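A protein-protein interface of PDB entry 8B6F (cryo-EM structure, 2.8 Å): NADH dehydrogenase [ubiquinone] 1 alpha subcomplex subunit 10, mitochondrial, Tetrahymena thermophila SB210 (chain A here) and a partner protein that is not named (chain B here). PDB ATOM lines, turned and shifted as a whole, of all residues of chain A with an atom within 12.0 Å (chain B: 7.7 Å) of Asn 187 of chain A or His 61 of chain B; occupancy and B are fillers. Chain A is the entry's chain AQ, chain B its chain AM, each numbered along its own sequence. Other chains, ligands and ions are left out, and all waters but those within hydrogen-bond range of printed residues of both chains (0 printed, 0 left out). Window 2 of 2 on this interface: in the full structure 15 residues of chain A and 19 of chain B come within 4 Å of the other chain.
Of the 11 printed residues of chain A, 4 touch a printed residue of chain B.
Along chain A the printed residues that touch a printed residue of chain B span positions 180 to 187.
Printed residues of chain B that touch a printed residue of chain A: Thr 58, Phe 59, Tyr 60 and His 61.
Hydrophobic or aromatic side chains of chain B within 4 Å of the printed part of chain A: Tyr 60 and His 61.
Among the printed residues, no Asp or Glu carboxylate lies within 4 Å of a Lys or Arg side-chain nitrogen of the other chain.
O of Phe 59 of chain B lies within hydrogen-bond range of ND2 of Asn 187 of chain A.
Among the printed residues, pairs that only touch across the chains: Ile 183 of chain A with Thr 58 of chain B, Ser 186 of chain A with Tyr 60 of chain B, Asn 187 of chain A with Tyr 60 of chain B, Arg 180 of chain A with Thr 58 of chain B, Asn 187 of chain A with His 61 of chain B and Ile 183 of chain A with Tyr 60 of chain B.
The backbone carbonyl oxygen (O) of Thr 58 of chain B lies within hydrogen-bond range of the backbone NH (N) of Leu 77 of chain B (3.0 Å).
The backbone carbonyl oxygen of Tyr 60 of chain B is in hydrogen-bond range of the side-chain hydroxyl of Thr 63 of chain B, at 2.6 Å.
The side-chain amino group (NZ) of Lys 219 of chain B is in hydrogen-bond range of the backbone carbonyl oxygen (O) of His 61 of chain B (2.5 Å).
The backbone carbonyl oxygen of Ile 183 of chain A lies close to the side-chain amide oxygen of Asn 187 of chain A, 3.2 Å away.
Printed residues of chain B within 4 Å of Ser 186 of chain A: Tyr 60.
Of the printed residues of chain B, Asn 187 of chain A touches Phe 59 (3.0 Å), Tyr 60 (3.4 Å) and His 61 (3.7 Å).
Thr 58 of chain B touches just these residues of chain A: Arg 180 (3.5 Å) and Ile 183 (3.2 Å).
Printed residues of chain A within 4 Å of Phe 59 of chain B: Asn 187.
Tyr 60 of chain B touches three residues of chain A.
His 61 of chain B touches just one residue of chain A: Asn 187 (3.7 Å).
No residue of chain A comes within 4 Å of Ser 62 of chain B.
No residue of chain A comes within 4 Å of Thr 63 of chain B.
Ile 65 of chain B touches none of the printed residues of chain A.
No residue of chain A comes within 4 Å of Leu 231 of chain B.
The nearest residue of chain A that does not touch His 61 of chain B is Lys 188 of chain A (4.5 Å).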
ATOM      1  N   ALA A 178      -1.127 -11.534 -20.309  1.00  0.00           N
ATOM      2  CA  ALA A 178      -0.608 -10.783 -21.447  1.00  0.00           C
ATOM      3  C   ALA A 178      -1.001  -9.312 -21.370  1.00  0.00           C
ATOM      4  O   ALA A 178      -0.205  -8.431 -21.716  1.00  0.00           O
ATOM      5  CB  ALA A 178      -1.105 -11.402 -22.752  1.00  0.00           C
ATOM      6  N   GLU A 179      -2.226  -9.025 -20.929  1.00  0.00           N
ATOM      7  CA  GLU A 179      -2.666  -7.637 -20.823  1.00  0.00           C
ATOM      8  C   GLU A 179      -1.783  -6.857 -19.858  1.00  0.00           C
ATOM      9  O   GLU A 179      -1.299  -5.768 -20.183  1.00  0.00           O
ATOM     10  CB  GLU A 179      -4.123  -7.579 -20.373  1.00  0.00           C
ATOM     11  CG  GLU A 179      -5.100  -8.218 -21.340  1.00  0.00           C
ATOM     12  CD  GLU A 179      -6.512  -8.250 -20.791  1.00  0.00           C
ATOM     13  OE1 GLU A 179      -6.669  -8.235 -19.552  1.00  0.00           O
ATOM     14  OE2 GLU A 179      -7.465  -8.283 -21.595  1.00  0.00           O
ATOM     15  N   ARG A 180      -1.561  -7.402 -18.661  1.00  0.00           N
ATOM     16  CA  ARG A 180      -0.719  -6.713 -17.690  1.00  0.00           C
ATOM     17  C   ARG A 180       0.705  -6.568 -18.204  1.00  0.00           C
ATOM     18  O   ARG A 180       1.325  -5.511 -18.045  1.00  0.00           O
ATOM     19  CB  ARG A 180      -0.734  -7.462 -16.360  1.00  0.00           C
ATOM     20  CG  ARG A 180       0.325  -6.991 -15.378  1.00  0.00           C
ATOM     21  CD  ARG A 180       0.074  -7.536 -13.986  1.00  0.00           C
ATOM     22  NE  ARG A 180       1.210  -7.310 -13.100  1.00  0.00           N
ATOM     23  CZ  ARG A 180       1.435  -6.192 -12.424  1.00  0.00           C
ATOM     24  NH1 ARG A 180       0.622  -5.154 -12.513  1.00  0.00           N
ATOM     25  NH2 ARG A 180       2.505  -6.113 -11.640  1.00  0.00           N
ATOM     26  N   GLU A 181       1.239  -7.614 -18.832  1.00  0.00           N
ATOM     27  CA  GLU A 181       2.596  -7.534 -19.361  1.00  0.00           C
ATOM     28  C   GLU A 181       2.712  -6.439 -20.413  1.00  0.00           C
ATOM     29  O   GLU A 181       3.675  -5.665 -20.411  1.00  0.00           O
ATOM     30  CB  GLU A 181       3.016  -8.884 -19.941  1.00  0.00           C
ATOM     31  CG  GLU A 181       3.247  -9.959 -18.890  1.00  0.00           C
ATOM     32  CD  GLU A 181       3.627 -11.297 -19.499  1.00  0.00           C
ATOM     33  OE1 GLU A 181       3.714 -11.382 -20.741  1.00  0.00           O
ATOM     34  OE2 GLU A 181       3.839 -12.262 -18.734  1.00  0.00           O
ATOM     35  N   ALA A 182       1.740  -6.359 -21.324  1.00  0.00           N
ATOM     36  CA  ALA A 182       1.796  -5.339 -22.366  1.00  0.00           C
ATOM     37  C   ALA A 182       1.691  -3.937 -21.777  1.00  0.00           C
ATOM     38  O   ALA A 182       2.420  -3.028 -22.191  1.00  0.00           O
ATOM     39  CB  ALA A 182       0.683  -5.573 -23.386  1.00  0.00           C
ATOM     40  N   ILE A 183       0.786  -3.739 -20.818  1.00  0.00           N
ATOM     41  CA  ILE A 183       0.626  -2.416 -20.221  1.00  0.00           C
ATOM     42  C   ILE A 183       1.886  -2.019 -19.464  1.00  0.00           C
ATOM     43  O   ILE A 183       2.331  -0.868 -19.535  1.00  0.00           O
ATOM     44  CB  ILE A 183      -0.622  -2.383 -19.320  1.00  0.00           C
ATOM     45  CG1 ILE A 183      -1.882  -2.582 -20.167  1.00  0.00           C
ATOM     46  CG2 ILE A 183      -0.701  -1.065 -18.558  1.00  0.00           C
ATOM     47  CD1 ILE A 183      -3.152  -2.761 -19.365  1.00  0.00           C
ATOM     48  N   LEU A 184       2.482  -2.960 -18.729  1.00  0.00           N
ATOM     49  CA  LEU A 184       3.722  -2.661 -18.023  1.00  0.00           C
ATOM     50  C   LEU A 184       4.844  -2.329 -18.996  1.00  0.00           C
ATOM     51  O   LEU A 184       5.639  -1.416 -18.750  1.00  0.00           O
ATOM     52  CB  LEU A 184       4.121  -3.837 -17.130  1.00  0.00           C
ATOM     53  CG  LEU A 184       3.221  -4.129 -15.928  1.00  0.00           C
ATOM     54  CD1 LEU A 184       3.718  -5.357 -15.192  1.00  0.00           C
ATOM     55  CD2 LEU A 184       3.149  -2.939 -14.983  1.00  0.00           C
ATOM     56  N   LYS A 185       4.931  -3.066 -20.104  1.00  0.00           N
ATOM     57  CA  LYS A 185       5.959  -2.776 -21.096  1.00  0.00           C
ATOM     58  C   LYS A 185       5.771  -1.384 -21.685  1.00  0.00           C
ATOM     59  O   LYS A 185       6.745  -0.652 -21.893  1.00  0.00           O
ATOM     60  CB  LYS A 185       5.934  -3.836 -22.198  1.00  0.00           C
ATOM     61  CG  LYS A 185       6.975  -3.635 -23.293  1.00  0.00           C
ATOM     62  CD  LYS A 185       8.394  -3.756 -22.756  1.00  0.00           C
ATOM     63  CE  LYS A 185       9.425  -3.515 -23.849  1.00  0.00           C
ATOM     64  NZ  LYS A 185       9.275  -4.459 -24.992  1.00  0.00           N
ATOM     65  N   SER A 186       4.524  -1.004 -21.970  1.00  0.00           N
ATOM     66  CA  SER A 186       4.264   0.333 -22.493  1.00  0.00           C
ATOM     67  C   SER A 186       4.620   1.406 -21.471  1.00  0.00           C
ATOM     68  O   SER A 186       5.189   2.445 -21.824  1.00  0.00           O
ATOM     69  CB  SER A 186       2.800   0.459 -22.911  1.00  0.00           C
ATOM     70  OG  SER A 186       2.549   1.741 -23.460  1.00  0.00           O
ATOM     71  N   ASN A 187       4.284   1.178 -20.200  1.00  0.00           N
ATOM     72  CA  ASN A 187       4.608   2.155 -19.165  1.00  0.00           C
ATOM     73  C   ASN A 187       6.113   2.326 -19.017  1.00  0.00           C
ATOM     74  O   ASN A 187       6.607   3.450 -18.878  1.00  0.00           O
ATOM     75  CB  ASN A 187       3.993   1.731 -17.831  1.00  0.00           C
ATOM     76  CG  ASN A 187       2.494   1.929 -17.791  1.00  0.00           C
ATOM     77  OD1 ASN A 187       1.865   2.194 -18.812  1.00  0.00           O
ATOM     78  ND2 ASN A 187       1.913   1.792 -16.606  1.00  0.00           N
ATOM     79  N   LYS A 188       6.858   1.225 -19.039  1.00  0.00           N
ATOM     80  CA  LYS A 188       8.300   1.266 -18.833  1.00  0.00           C
ATOM     81  C   LYS A 188       8.627   1.910 -17.492  1.00  0.00           C
ATOM     82  O   LYS A 188       7.786   1.955 -16.594  1.00  0.00           O
ATOM     83  CB  LYS A 188       8.992   2.026 -19.968  1.00  0.00           C
ATOM     84  CG  LYS A 188       8.752   1.426 -21.345  1.00  0.00           C
ATOM     85  CD  LYS A 188       9.573   2.132 -22.412  1.00  0.00           C
ATOM     86  CE  LYS A 188       9.389   1.474 -23.771  1.00  0.00           C
ATOM     87  NZ  LYS A 188      10.217   2.127 -24.823  1.00  0.00           N
ATOM     88  N   THR B  58      -3.837  -2.470 -13.386  1.00  0.00           N
ATOM     89  CA  THR B  58      -2.873  -1.993 -14.367  1.00  0.00           C
ATOM     90  C   THR B  58      -3.495  -0.855 -15.158  1.00  0.00           C
ATOM     91  O   THR B  58      -4.642  -0.962 -15.606  1.00  0.00           O
ATOM     92  CB  THR B  58      -2.435  -3.110 -15.317  1.00  0.00           C
ATOM     93  OG1 THR B  58      -3.467  -3.356 -16.280  1.00  0.00           O
ATOM     94  CG2 THR B  58      -2.164  -4.386 -14.547  1.00  0.00           C
ATOM     95  N   PHE B  59      -2.742   0.224 -15.331  1.00  0.00           N
ATOM     96  CA  PHE B  59      -3.242   1.392 -16.036  1.00  0.00           C
ATOM     97  C   PHE B  59      -2.064   2.164 -16.608  1.00  0.00           C
ATOM     98  O   PHE B  59      -1.008   2.248 -15.980  1.00  0.00           O
ATOM     99  CB  PHE B  59      -4.066   2.285 -15.101  1.00  0.00           C
ATOM    100  CG  PHE B  59      -3.393   2.572 -13.795  1.00  0.00           C
ATOM    101  CD1 PHE B  59      -2.549   3.658 -13.659  1.00  0.00           C
ATOM    102  CD2 PHE B  59      -3.606   1.751 -12.700  1.00  0.00           C
ATOM    103  CE1 PHE B  59      -1.929   3.924 -12.456  1.00  0.00           C
ATOM    104  CE2 PHE B  59      -2.989   2.010 -11.493  1.00  0.00           C
ATOM    105  CZ  PHE B  59      -2.149   3.098 -11.370  1.00  0.00           C
ATOM    106  N   TYR B  60      -2.254   2.715 -17.804  1.00  0.00           N
ATOM    107  CA  TYR B  60      -1.229   3.554 -18.404  1.00  0.00           C
ATOM    108  C   TYR B  60      -1.026   4.811 -17.569  1.00  0.00           C
ATOM    109  O   TYR B  60      -1.975   5.368 -17.013  1.00  0.00           O
ATOM    110  CB  TYR B  60      -1.626   3.936 -19.830  1.00  0.00           C
ATOM    111  CG  TYR B  60      -1.646   2.773 -20.795  1.00  0.00           C
ATOM    112  CD1 TYR B  60      -2.733   1.911 -20.851  1.00  0.00           C
ATOM    113  CD2 TYR B  60      -0.583   2.541 -21.654  1.00  0.00           C
ATOM    114  CE1 TYR B  60      -2.758   0.850 -21.733  1.00  0.00           C
ATOM    115  CE2 TYR B  60      -0.600   1.482 -22.539  1.00  0.00           C
ATOM    116  CZ  TYR B  60      -1.689   0.641 -22.574  1.00  0.00           C
ATOM    117  OH  TYR B  60      -1.701  -0.413 -23.456  1.00  0.00           O
ATOM    118  N   HIS B  61       0.227   5.261 -17.485  1.00  0.00           N
ATOM    119  CA  HIS B  61       0.527   6.458 -16.709  1.00  0.00           C
ATOM    120  C   HIS B  61      -0.223   7.679 -17.219  1.00  0.00           C
ATOM    121  O   HIS B  61      -0.399   8.644 -16.468  1.00  0.00           O
ATOM    122  CB  HIS B  61       2.032   6.729 -16.724  1.00  0.00           C
ATOM    123  CG  HIS B  61       2.821   5.803 -15.853  1.00  0.00           C
ATOM    124  ND1 HIS B  61       4.180   5.623 -15.997  1.00  0.00           N
ATOM    125  CD2 HIS B  61       2.443   5.008 -14.823  1.00  0.00           C
ATOM    126  CE1 HIS B  61       4.604   4.756 -15.095  1.00  0.00           C
ATOM    127  NE2 HIS B  61       3.571   4.368 -14.371  1.00  0.00           N
ATOM    128  N   SER B  62      -0.667   7.662 -18.476  1.00  0.00           N
ATOM    129  CA  SER B  62      -1.432   8.779 -19.012  1.00  0.00           C
ATOM    130  C   SER B  62      -2.818   8.891 -18.393  1.00  0.00           C
ATOM    131  O   SER B  62      -3.423   9.966 -18.453  1.00  0.00           O
ATOM    132  CB  SER B  62      -1.551   8.637 -20.529  1.00  0.00           C
ATOM    133  OG  SER B  62      -2.453   9.591 -21.060  1.00  0.00           O
ATOM    134  N   THR B  63      -3.335   7.816 -17.805  1.00  0.00           N
ATOM    135  CA  THR B  63      -4.672   7.842 -17.231  1.00  0.00           C
ATOM    136  C   THR B  63      -4.735   8.761 -16.018  1.00  0.00           C
ATOM    137  O   THR B  63      -3.770   8.899 -15.262  1.00  0.00           O
ATOM    138  CB  THR B  63      -5.106   6.437 -16.816  1.00  0.00           C
ATOM    139  OG1 THR B  63      -4.240   5.953 -15.782  1.00  0.00           O
ATOM    140  CG2 THR B  63      -5.056   5.490 -17.996  1.00  0.00           C
ATOM    141  N   PHE B  64      -5.891   9.391 -15.832  1.00  0.00           N
ATOM    142  CA  PHE B  64      -6.178  10.171 -14.636  1.00  0.00           C
ATOM    143  C   PHE B  64      -7.110   9.363 -13.741  1.00  0.00           C
ATOM    144  O   PHE B  64      -8.237   9.051 -14.135  1.00  0.00           O
ATOM    145  CB  PHE B  64      -6.797  11.524 -14.984  1.00  0.00           C
ATOM    146  CG  PHE B  64      -7.443  12.206 -13.814  1.00  0.00           C
ATOM    147  CD1 PHE B  64      -6.706  12.518 -12.685  1.00  0.00           C
ATOM    148  CD2 PHE B  64      -8.780  12.544 -13.846  1.00  0.00           C
ATOM    149  CE1 PHE B  64      -7.298  13.146 -11.609  1.00  0.00           C
ATOM    150  CE2 PHE B  64      -9.378  13.169 -12.775  1.00  0.00           C
ATOM    151  CZ  PHE B  64      -8.636  13.472 -11.654  1.00  0.00           C
ATOM    152  N   ILE B  65      -6.639   9.030 -12.544  1.00  0.00           N
ATOM    153  CA  ILE B  65      -7.402   8.269 -11.564  1.00  0.00           C
ATOM    154  C   ILE B  65      -7.615   9.168 -10.355  1.00  0.00           C
ATOM    155  O   ILE B  65      -6.645   9.612  -9.728  1.00  0.00           O
ATOM    156  CB  ILE B  65      -6.684   6.969 -11.168  1.00  0.00           C
ATOM    157  CG1 ILE B  65      -6.494   6.075 -12.395  1.00  0.00           C
ATOM    158  CG2 ILE B  65      -7.470   6.227 -10.093  1.00  0.00           C
ATOM    159  CD1 ILE B  65      -5.589   4.891 -12.157  1.00  0.00           C
ATOM    160  N   LEU B  77      -7.036  -0.319 -17.247  1.00  0.00           N
ATOM    161  CA  LEU B  77      -7.412   0.958 -17.832  1.00  0.00           C
ATOM    162  C   LEU B  77      -6.586   1.222 -19.083  1.00  0.00           C
ATOM    163  O   LEU B  77      -5.461   0.735 -19.222  1.00  0.00           O
ATOM    164  CB  LEU B  77      -7.222   2.102 -16.834  1.00  0.00           C
ATOM    165  CG  LEU B  77      -8.030   2.007 -15.538  1.00  0.00           C
ATOM    166  CD1 LEU B  77      -7.750   3.205 -14.652  1.00  0.00           C
ATOM    167  CD2 LEU B  77      -9.516   1.891 -15.818  1.00  0.00           C
ATOM    168  N   GLY B  78      -7.156   2.006 -19.987  1.00  0.00           N
ATOM    169  CA  GLY B  78      -6.548   2.296 -21.266  1.00  0.00           C
ATOM    170  C   GLY B  78      -5.570   3.447 -21.203  1.00  0.00           C
ATOM    171  O   GLY B  78      -4.995   3.757 -20.156  1.00  0.00           O
ATOM    172  N   GLN B  79      -5.379   4.091 -22.353  1.00  0.00           N
ATOM    173  CA  GLN B  79      -4.367   5.135 -22.469  1.00  0.00           C
ATOM    174  C   GLN B  79      -4.746   6.365 -21.653  1.00  0.00           C
ATOM    175  O   GLN B  79      -4.025   6.757 -20.729  1.00  0.00           O
ATOM    176  CB  GLN B  79      -4.170   5.502 -23.940  1.00  0.00           C
ATOM    177  CG  GLN B  79      -2.990   6.422 -24.198  1.00  0.00           C
ATOM    178  CD  GLN B  79      -1.662   5.774 -23.872  1.00  0.00           C
ATOM    179  OE1 GLN B  79      -1.583   4.564 -23.670  1.00  0.00           O
ATOM    180  NE2 GLN B  79      -0.608   6.579 -23.815  1.00  0.00           N
ATOM    181  N   ASN B  80      -5.878   6.991 -21.976  1.00  0.00           N
ATOM    182  CA  ASN B  80      -6.277   8.252 -21.361  1.00  0.00           C
ATOM    183  C   ASN B  80      -7.583   8.116 -20.583  1.00  0.00           C
ATOM    184  O   ASN B  80      -8.325   9.087 -20.432  1.00  0.00           O
ATOM    185  CB  ASN B  80      -6.406   9.344 -22.421  1.00  0.00           C
ATOM    186  CG  ASN B  80      -5.149   9.500 -23.249  1.00  0.00           C
ATOM    187  OD1 ASN B  80      -4.220  10.205 -22.861  1.00  0.00           O
ATOM    188  ND2 ASN B  80      -5.114   8.839 -24.400  1.00  0.00           N
ATOM    189  N   LYS B 219      -5.799  16.287 -13.352  1.00  0.00           N
ATOM    190  CA  LYS B 219      -4.563  15.598 -13.001  1.00  0.00           C
ATOM    191  C   LYS B 219      -3.431  16.595 -12.783  1.00  0.00           C
ATOM    192  O   LYS B 219      -2.682  16.499 -11.805  1.00  0.00           O
ATOM    193  CB  LYS B 219      -4.200  14.594 -14.094  1.00  0.00           C
ATOM    194  CG  LYS B 219      -3.004  13.718 -13.763  1.00  0.00           C
ATOM    195  CD  LYS B 219      -2.741  12.719 -14.877  1.00  0.00           C
ATOM    196  CE  LYS B 219      -1.583  11.802 -14.536  1.00  0.00           C
ATOM    197  NZ  LYS B 219      -1.297  10.841 -15.635  1.00  0.00           N
ATOM    198  N   ILE B 223      -1.575  17.199  -9.156  1.00  0.00           N
ATOM    199  CA  ILE B 223      -0.131  17.013  -9.034  1.00  0.00           C
ATOM    200  C   ILE B 223       0.514  18.289  -8.514  1.00  0.00           C
ATOM    201  O   ILE B 223       1.435  18.247  -7.690  1.00  0.00           O
ATOM    202  CB  ILE B 223       0.470  16.578 -10.385  1.00  0.00           C
ATOM    203  CG1 ILE B 223      -0.020  15.176 -10.757  1.00  0.00           C
ATOM    204  CG2 ILE B 223       1.996  16.611 -10.337  1.00  0.00           C
ATOM    205  CD1 ILE B 223       0.317  14.758 -12.175  1.00  0.00           C
ATOM    206  N   TYR B 228      -2.016  14.300  -5.839  1.00  0.00           N
ATOM    207  CA  TYR B 228      -1.884  13.192  -6.773  1.00  0.00           C
ATOM    208  C   TYR B 228      -0.474  12.630  -6.674  1.00  0.00           C
ATOM    209  O   TYR B 228       0.503  13.376  -6.780  1.00  0.00           O
ATOM    210  CB  TYR B 228      -2.175  13.658  -8.203  1.00  0.00           C
ATOM    211  CG  TYR B 228      -2.504  12.548  -9.169  1.00  0.00           C
ATOM    212  CD1 TYR B 228      -1.496  11.802  -9.758  1.00  0.00           C
ATOM    213  CD2 TYR B 228      -3.819  12.259  -9.505  1.00  0.00           C
ATOM    214  CE1 TYR B 228      -1.784  10.791 -10.646  1.00  0.00           C
ATOM    215  CE2 TYR B 228      -4.119  11.247 -10.395  1.00  0.00           C
ATOM    216  CZ  TYR B 228      -3.093  10.517 -10.961  1.00  0.00           C
ATOM    217  OH  TYR B 228      -3.364   9.506 -11.850  1.00  0.00           O
ATOM    218  N   ARG B 230       2.797  10.947  -7.890  1.00  0.00           N
ATOM    219  CA  ARG B 230       3.499  10.890  -9.171  1.00  0.00           C
ATOM    220  C   ARG B 230       3.975   9.459  -9.397  1.00  0.00           C
ATOM    221  O   ARG B 230       5.111   9.083  -9.099  1.00  0.00           O
ATOM    222  CB  ARG B 230       4.654  11.882  -9.191  1.00  0.00           C
ATOM    223  CG  ARG B 230       4.231  13.310  -8.883  1.00  0.00           C
ATOM    224  CD  ARG B 230       5.424  14.249  -8.841  1.00  0.00           C
ATOM    225  NE  ARG B 230       5.033  15.596  -8.445  1.00  0.00           N
ATOM    226  CZ  ARG B 230       5.874  16.611  -8.305  1.00  0.00           C
ATOM    227  NH1 ARG B 230       7.172  16.470  -8.524  1.00  0.00           N
ATOM    228  NH2 ARG B 230       5.403  17.799  -7.935  1.00  0.00           N
ATOM    229  N   LEU B 231       3.076   8.646  -9.942  1.00  0.00           N
ATOM    230  CA  LEU B 231       3.362   7.240 -10.199  1.00  0.00           C
ATOM    231  C   LEU B 231       4.476   7.087 -11.227  1.00  0.00           C
ATOM    232  O   LEU B 231       5.657   7.183 -10.896  1.00  0.00           O
ATOM    233  CB  LEU B 231       2.099   6.523 -10.681  1.00  0.00           C
ATOM    234  CG  LEU B 231       0.902   6.588  -9.728  1.00  0.00           C
ATOM    235  CD1 LEU B 231      -0.344   6.045 -10.396  1.00  0.00           C
ATOM    236  CD2 LEU B 231       1.191   5.823  -8.446  1.00  0.00           C
